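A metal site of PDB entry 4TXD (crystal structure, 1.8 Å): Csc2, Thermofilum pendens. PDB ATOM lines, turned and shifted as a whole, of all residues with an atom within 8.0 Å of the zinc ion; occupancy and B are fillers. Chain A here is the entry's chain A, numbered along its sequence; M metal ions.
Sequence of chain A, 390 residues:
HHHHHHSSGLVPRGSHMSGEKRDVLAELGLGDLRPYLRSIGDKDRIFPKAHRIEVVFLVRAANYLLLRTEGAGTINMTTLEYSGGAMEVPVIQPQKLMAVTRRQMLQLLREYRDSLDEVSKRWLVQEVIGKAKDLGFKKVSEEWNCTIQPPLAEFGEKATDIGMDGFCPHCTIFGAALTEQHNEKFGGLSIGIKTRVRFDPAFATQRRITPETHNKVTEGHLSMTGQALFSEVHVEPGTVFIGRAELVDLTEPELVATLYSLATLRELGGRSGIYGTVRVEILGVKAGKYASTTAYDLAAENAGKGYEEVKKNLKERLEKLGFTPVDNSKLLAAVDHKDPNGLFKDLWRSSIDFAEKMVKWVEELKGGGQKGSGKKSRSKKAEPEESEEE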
ATOM      1  N   ARG A 102      32.858   8.951  14.313  1.00  0.00           N
ATOM      2  CA  ARG A 102      31.949   9.650  13.458  1.00  0.00           C
ATOM      3  C   ARG A 102      30.653   8.895  13.279  1.00  0.00           C
ATOM      4  O   ARG A 102      29.612   9.457  13.232  1.00  0.00           O
ATOM      5  CB  ARG A 102      32.606  10.046  12.142  1.00  0.00           C
ATOM      6  CG  ARG A 102      32.274   9.246  10.964  1.00  0.00           C
ATOM      7  CD  ARG A 102      32.034  10.128   9.762  1.00  0.00           C
ATOM      8  NE  ARG A 102      33.276  10.434   9.101  1.00  0.00           N
ATOM      9  CZ  ARG A 102      33.544  11.522   8.398  1.00  0.00           C
ATOM     10  NH1 ARG A 102      34.719  11.617   7.876  1.00  0.00           N
ATOM     11  NH2 ARG A 102      32.687  12.510   8.229  1.00  0.00           N
ATOM     12  N   LEU A 106      26.953  10.307  14.364  1.00  0.00           N
ATOM     13  CA  LEU A 106      25.869  10.160  13.452  1.00  0.00           C
ATOM     14  C   LEU A 106      24.656   9.485  14.106  1.00  0.00           C
ATOM     15  O   LEU A 106      23.529   9.848  13.862  1.00  0.00           O
ATOM     16  CB  LEU A 106      26.329   9.413  12.227  1.00  0.00           C
ATOM     17  CG  LEU A 106      25.253   9.097  11.219  1.00  0.00           C
ATOM     18  CD1 LEU A 106      24.380  10.306  10.939  1.00  0.00           C
ATOM     19  CD2 LEU A 106      25.766   8.488   9.952  1.00  0.00           C
ATOM     20  N   LEU A 109      23.064  11.928  16.353  1.00  0.00           N
ATOM     21  CA  LEU A 109      22.287  12.873  15.537  1.00  0.00           C
ATOM     22  C   LEU A 109      20.958  12.288  15.111  1.00  0.00           C
ATOM     23  O   LEU A 109      19.937  12.993  15.062  1.00  0.00           O
ATOM     24  CB  LEU A 109      23.079  13.294  14.277  1.00  0.00           C
ATOM     25  CG  LEU A 109      24.222  14.252  14.539  1.00  0.00           C
ATOM     26  CD1 LEU A 109      25.150  14.336  13.312  1.00  0.00           C
ATOM     27  CD2 LEU A 109      23.675  15.633  14.911  1.00  0.00           C
ATOM     28  N   LYS A 139      21.058  17.416  -0.644  1.00  0.00           N
ATOM     29  CA  LYS A 139      20.457  16.458   0.245  1.00  0.00           C
ATOM     30  C   LYS A 139      19.625  17.143   1.314  1.00  0.00           C
ATOM     31  O   LYS A 139      19.993  17.182   2.450  1.00  0.00           O
ATOM     32  CB  LYS A 139      21.525  15.580   0.856  1.00  0.00           C
ATOM     33  CG  LYS A 139      21.928  14.461  -0.057  1.00  0.00           C
ATOM     34  CD  LYS A 139      22.845  14.875  -1.199  1.00  0.00           C
ATOM     35  CE  LYS A 139      23.278  13.698  -2.053  1.00  0.00           C
ATOM     36  NZ  LYS A 139      24.431  12.971  -1.474  1.00  0.00           N
ATOM     37  N   TRP A 144      15.451  14.295   7.713  1.00  0.00           N
ATOM     38  CA  TRP A 144      16.895  14.325   7.675  1.00  0.00           C
ATOM     39  C   TRP A 144      17.571  12.973   7.870  1.00  0.00           C
ATOM     40  O   TRP A 144      17.220  12.226   8.729  1.00  0.00           O
ATOM     41  CB  TRP A 144      17.507  15.342   8.643  1.00  0.00           C
ATOM     42  CG  TRP A 144      18.993  15.317   8.615  1.00  0.00           C
ATOM     43  CD1 TRP A 144      19.806  15.928   7.723  1.00  0.00           C
ATOM     44  CD2 TRP A 144      19.833  14.550   9.456  1.00  0.00           C
ATOM     45  NE1 TRP A 144      21.110  15.635   7.985  1.00  0.00           N
ATOM     46  CE2 TRP A 144      21.154  14.782   9.035  1.00  0.00           C
ATOM     47  CE3 TRP A 144      19.601  13.714  10.523  1.00  0.00           C
ATOM     48  CZ2 TRP A 144      22.228  14.196   9.667  1.00  0.00           C
ATOM     49  CZ3 TRP A 144      20.655  13.136  11.132  1.00  0.00           C
ATOM     50  CH2 TRP A 144      21.961  13.377  10.710  1.00  0.00           C
ATOM     51  N   ASN A 145      18.602  12.752   7.078  1.00  0.00           N
ATOM     52  CA  ASN A 145      19.514  11.667   7.392  1.00  0.00           C
ATOM     53  C   ASN A 145      20.829  11.932   6.688  1.00  0.00           C
ATOM     54  O   ASN A 145      20.885  12.716   5.731  1.00  0.00           O
ATOM     55  CB  ASN A 145      18.939  10.315   6.982  1.00  0.00           C
ATOM     56  CG  ASN A 145      19.656   9.143   7.660  1.00  0.00           C
ATOM     57  OD1 ASN A 145      20.245   9.290   8.733  1.00  0.00           O
ATOM     58  ND2 ASN A 145      19.601   7.986   7.024  1.00  0.00           N
ATOM     59  N   CYS A 146      21.885  11.316   7.183  1.00  0.00           N
ATOM     60  CA  CYS A 146      23.186  11.347   6.536  1.00  0.00           C
ATOM     61  C   CYS A 146      23.807   9.968   6.674  1.00  0.00           C
ATOM     62  O   CYS A 146      23.428   9.188   7.559  1.00  0.00           O
ATOM     63  CB  CYS A 146      24.081  12.442   7.133  1.00  0.00           C
ATOM     64  SG  CYS A 146      25.641  12.819   6.205  1.00  0.00           S
ATOM     65  N   THR A 147      24.758   9.658   5.838  1.00  0.00           N
ATOM     66  CA  THR A 147      25.470   8.431   6.031  1.00  0.00           C
ATOM     67  C   THR A 147      26.860   8.690   6.513  1.00  0.00           C
ATOM     68  O   THR A 147      27.308   9.809   6.594  1.00  0.00           O
ATOM     69  CB  THR A 147      25.596   7.645   4.761  1.00  0.00           C
ATOM     70  OG1 THR A 147      26.319   6.478   5.070  1.00  0.00           O
ATOM     71  CG2 THR A 147      26.339   8.421   3.731  1.00  0.00           C
ATOM     72  N   ILE A 148      27.568   7.612   6.787  1.00  0.00           N
ATOM     73  CA  ILE A 148      28.969   7.714   7.053  1.00  0.00           C
ATOM     74  C   ILE A 148      29.723   7.285   5.805  1.00  0.00           C
ATOM     75  O   ILE A 148      30.921   7.336   5.774  1.00  0.00           O
ATOM     76  CB  ILE A 148      29.395   6.873   8.280  1.00  0.00           C
ATOM     77  N   GLY A 163      23.647   9.607   0.096  1.00  0.00           N
ATOM     78  CA  GLY A 163      25.044   9.788   0.448  1.00  0.00           C
ATOM     79  C   GLY A 163      25.209  10.719   1.635  1.00  0.00           C
ATOM     80  O   GLY A 163      24.277  10.912   2.414  1.00  0.00           O
ATOM     81  N   MET A 164      26.400  11.312   1.772  1.00  0.00           N
ATOM     82  CA  MET A 164      26.667  12.287   2.806  1.00  0.00           C
ATOM     83  C   MET A 164      26.038  13.598   2.395  1.00  0.00           C
ATOM     84  O   MET A 164      25.932  13.851   1.227  1.00  0.00           O
ATOM     85  CB  MET A 164      28.175  12.433   3.019  1.00  0.00           C
ATOM     86  CG  MET A 164      28.806  11.329   3.840  1.00  0.00           C
ATOM     87  SD  MET A 164      30.597  11.179   3.830  1.00  0.00           S
ATOM     88  CE  MET A 164      31.036  12.333   5.097  1.00  0.00           C
ATOM     89  N   ASP A 165      25.616  14.412   3.349  1.00  0.00           N
ATOM     90  CA  ASP A 165      24.974  15.660   3.006  1.00  0.00           C
ATOM     91  C   ASP A 165      25.930  16.832   2.858  1.00  0.00           C
ATOM     92  O   ASP A 165      25.664  17.766   2.166  1.00  0.00           O
ATOM     93  CB  ASP A 165      23.841  15.997   3.975  1.00  0.00           C
ATOM     94  CG  ASP A 165      24.279  15.991   5.407  1.00  0.00           C
ATOM     95  OD1 ASP A 165      25.418  16.233   5.695  1.00  0.00           O
ATOM     96  OD2 ASP A 165      23.446  15.751   6.270  1.00  0.00           O
ATOM     97  N   GLY A 166      27.059  16.736   3.520  1.00  0.00           N
ATOM     98  CA  GLY A 166      28.043  17.769   3.478  1.00  0.00           C
ATOM     99  C   GLY A 166      27.785  18.967   4.341  1.00  0.00           C
ATOM    100  O   GLY A 166      28.504  19.909   4.266  1.00  0.00           O
ATOM    101  N   PHE A 167      26.755  18.905   5.183  1.00  0.00           N
ATOM    102  CA  PHE A 167      26.485  20.010   6.065  1.00  0.00           C
ATOM    103  C   PHE A 167      26.140  19.660   7.509  1.00  0.00           C
ATOM    104  O   PHE A 167      26.072  20.508   8.311  1.00  0.00           O
ATOM    105  CB  PHE A 167      25.445  20.952   5.465  1.00  0.00           C
ATOM    106  CG  PHE A 167      24.089  20.350   5.348  1.00  0.00           C
ATOM    107  CD1 PHE A 167      23.246  20.348   6.407  1.00  0.00           C
ATOM    108  CD2 PHE A 167      23.671  19.771   4.210  1.00  0.00           C
ATOM    109  CE1 PHE A 167      22.002  19.799   6.323  1.00  0.00           C
ATOM    110  CE2 PHE A 167      22.431  19.213   4.098  1.00  0.00           C
ATOM    111  CZ  PHE A 167      21.592  19.231   5.165  1.00  0.00           C
ATOM    112  N   CYS A 168      25.940  18.394   7.781  1.00  0.00           N
ATOM    113  CA  CYS A 168      25.650  17.961   9.123  1.00  0.00           C
ATOM    114  C   CYS A 168      26.899  17.957   9.990  1.00  0.00           C
ATOM    115  O   CYS A 168      27.979  18.020   9.522  1.00  0.00           O
ATOM    116  CB  CYS A 168      24.956  16.620   9.121  1.00  0.00           C
ATOM    117  SG  CYS A 168      26.039  15.197   9.116  1.00  0.00           S
ATOM    118  N   PRO A 169      26.608  17.926  11.362  1.00  0.00           N
ATOM    119  CA  PRO A 169      27.794  17.985  12.211  1.00  0.00           C
ATOM    120  C   PRO A 169      28.871  16.928  11.958  1.00  0.00           C
ATOM    121  O   PRO A 169      29.997  17.230  12.082  1.00  0.00           O
ATOM    122  CB  PRO A 169      27.231  17.821  13.611  1.00  0.00           C
ATOM    123  CG  PRO A 169      25.909  18.471  13.555  1.00  0.00           C
ATOM    124  CD  PRO A 169      25.386  17.961  12.302  1.00  0.00           C
ATOM    125  N   HIS A 170      28.509  15.711  11.620  1.00  0.00           N
ATOM    126  CA  HIS A 170      29.544  14.728  11.422  1.00  0.00           C
ATOM    127  C   HIS A 170      30.331  15.018  10.152  1.00  0.00           C
ATOM    128  O   HIS A 170      31.495  14.853  10.141  1.00  0.00           O
ATOM    129  CB  HIS A 170      29.037  13.297  11.520  1.00  0.00           C
ATOM    130  CG  HIS A 170      28.743  12.644  10.221  1.00  0.00           C
ATOM    131  ND1 HIS A 170      29.720  12.165   9.405  1.00  0.00           N
ATOM    132  CD2 HIS A 170      27.577  12.413   9.605  1.00  0.00           C
ATOM    133  CE1 HIS A 170      29.174  11.650   8.327  1.00  0.00           C
ATOM    134  NE2 HIS A 170      27.868  11.797   8.417  1.00  0.00           N
ATOM    135  N   CYS A 171      29.669  15.506   9.136  1.00  0.00           N
ATOM    136  CA  CYS A 171      30.373  15.906   7.924  1.00  0.00           C
ATOM    137  C   CYS A 171      31.303  17.071   8.136  1.00  0.00           C
ATOM    138  O   CYS A 171      32.406  17.025   7.724  1.00  0.00           O
ATOM    139  CB  CYS A 171      29.396  16.237   6.805  1.00  0.00           C
ATOM    140  SG  CYS A 171      28.572  14.850   6.044  1.00  0.00           S
ATOM    141  N   THR A 172      30.835  18.095   8.798  1.00  0.00           N
ATOM    142  CA  THR A 172      31.610  19.292   8.954  1.00  0.00           C
ATOM    143  C   THR A 172      32.750  19.143   9.936  1.00  0.00           C
ATOM    144  O   THR A 172      33.754  19.767   9.808  1.00  0.00           O
ATOM    145  CB  THR A 172      30.750  20.506   9.287  1.00  0.00           C
ATOM    146  OG1 THR A 172      30.111  20.314  10.530  1.00  0.00           O
ATOM    147  CG2 THR A 172      29.716  20.708   8.238  1.00  0.00           C
ATOM    148  N   GLY A 175      34.931  15.744   8.388  1.00  0.00           N
ATOM    149  CA  GLY A 175      35.345  15.890   7.009  1.00  0.00           C
ATOM    150  C   GLY A 175      34.544  15.154   5.953  1.00  0.00           C
ATOM    151  O   GLY A 175      33.807  14.208   6.225  1.00  0.00           O
ATOM    152  N   ALA A 176      34.716  15.603   4.707  1.00  0.00           N
ATOM    153  CA  ALA A 176      33.979  15.046   3.583  1.00  0.00           C
ATOM    154  C   ALA A 176      34.584  15.516   2.278  1.00  0.00           C
ATOM    155  O   ALA A 176      35.186  16.595   2.209  1.00  0.00           O
ATOM    156  CB  ALA A 176      32.489  15.443   3.647  1.00  0.00           C
ATOM    157  N   LEU A 178      33.369  16.783  -1.128  1.00  0.00           N
ATOM    158  CA  LEU A 178      32.137  17.289  -1.726  1.00  0.00           C
ATOM    159  C   LEU A 178      32.306  17.650  -3.208  1.00  0.00           C
ATOM    160  O   LEU A 178      33.374  18.093  -3.633  1.00  0.00           O
ATOM    161  CB  LEU A 178      31.628  18.509  -0.956  1.00  0.00           C
ATOM    162  CG  LEU A 178      31.407  18.273   0.545  1.00  0.00           C
ATOM    163  CD1 LEU A 178      30.852  19.539   1.219  1.00  0.00           C
ATOM    164  CD2 LEU A 178      30.491  17.064   0.767  1.00  0.00           C
ATOM    165  N   TRP A 348      23.919  21.724  15.749  1.00  0.00           N
ATOM    166  CA  TRP A 348      23.368  21.896  14.409  1.00  0.00           C
ATOM    167  C   TRP A 348      23.510  23.359  13.959  1.00  0.00           C
ATOM    168  O   TRP A 348      23.940  23.624  12.868  1.00  0.00           O
ATOM    169  CB  TRP A 348      21.925  21.435  14.352  1.00  0.00           C
ATOM    170  CG  TRP A 348      21.654  20.110  13.792  1.00  0.00           C
ATOM    171  CD1 TRP A 348      21.077  19.088  14.433  1.00  0.00           C
ATOM    172  CD2 TRP A 348      21.853  19.667  12.458  1.00  0.00           C
ATOM    173  NE1 TRP A 348      20.918  18.041  13.627  1.00  0.00           N
ATOM    174  CE2 TRP A 348      21.391  18.354  12.392  1.00  0.00           C
ATOM    175  CE3 TRP A 348      22.394  20.248  11.313  1.00  0.00           C
ATOM    176  CZ2 TRP A 348      21.442  17.629  11.244  1.00  0.00           C
ATOM    177  CZ3 TRP A 348      22.443  19.512  10.193  1.00  0.00           C
ATOM    178  CH2 TRP A 348      21.982  18.230  10.149  1.00  0.00           C
ATOM    179  N   SER A 351      26.989  23.773  12.874  1.00  0.00           N
ATOM    180  CA  SER A 351      27.356  23.066  11.684  1.00  0.00           C
ATOM    181  C   SER A 351      26.890  23.821  10.458  1.00  0.00           C
ATOM    182  O   SER A 351      27.601  23.937   9.524  1.00  0.00           O
ATOM    183  CB  SER A 351      26.786  21.659  11.663  1.00  0.00           C
ATOM    184  OG  SER A 351      27.317  20.868  10.656  1.00  0.00           O
HETATM  185 ZN    ZN M   1      26.390  14.761   6.993  1.00  0.00          ZN
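NE1 of Trp 144 is in hydrogen-bond range of OD2 of Asp 165.
The side-chain sulfur of Cys 168 lies close to the backbone NH of His 170.
The backbone carbonyl oxygen (O) of Cys 168 is in hydrogen-bond range of the side-chain hydroxyl (OG1) of Thr 172, 3.3 Å away.
OG of Ser 351 lies close to O of Cys 168 (3.1 Å).
The side-chain sulfur of Cys 146 sits close to a ring nitrogen (NE2) of His 170 (3.3 Å).
The side-chain sulfur (SG) of Cys 171 lies close to the backbone NH (N) of Gly 166, at 3.5 Å.
The backbone carbonyl oxygen (O) of Thr 147 lies within hydrogen-bond range of a ring nitrogen (NE2) of His 170, at 2.8 Å.
A ring nitrogen (ND1) of His 170 lies close to the guanidinium group (NH2) of Arg 102 (3.2 Å).
Residues that only touch the zinc ion: His 170 (3.6 Å).
Five residues have an atom within 4 Å of the zinc ion: Cys 146, Asp 165, Cys 168, His 170 and Cys 171.
The zinc ion is bound by OD1 of Asp 165.
SG of Cys 168 binds the zinc ion, at 2.2 Å.
SG of Cys 146 is bound to the zinc ion.
SG of Cys 171 is bound to the zinc ion (2.4 Å).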
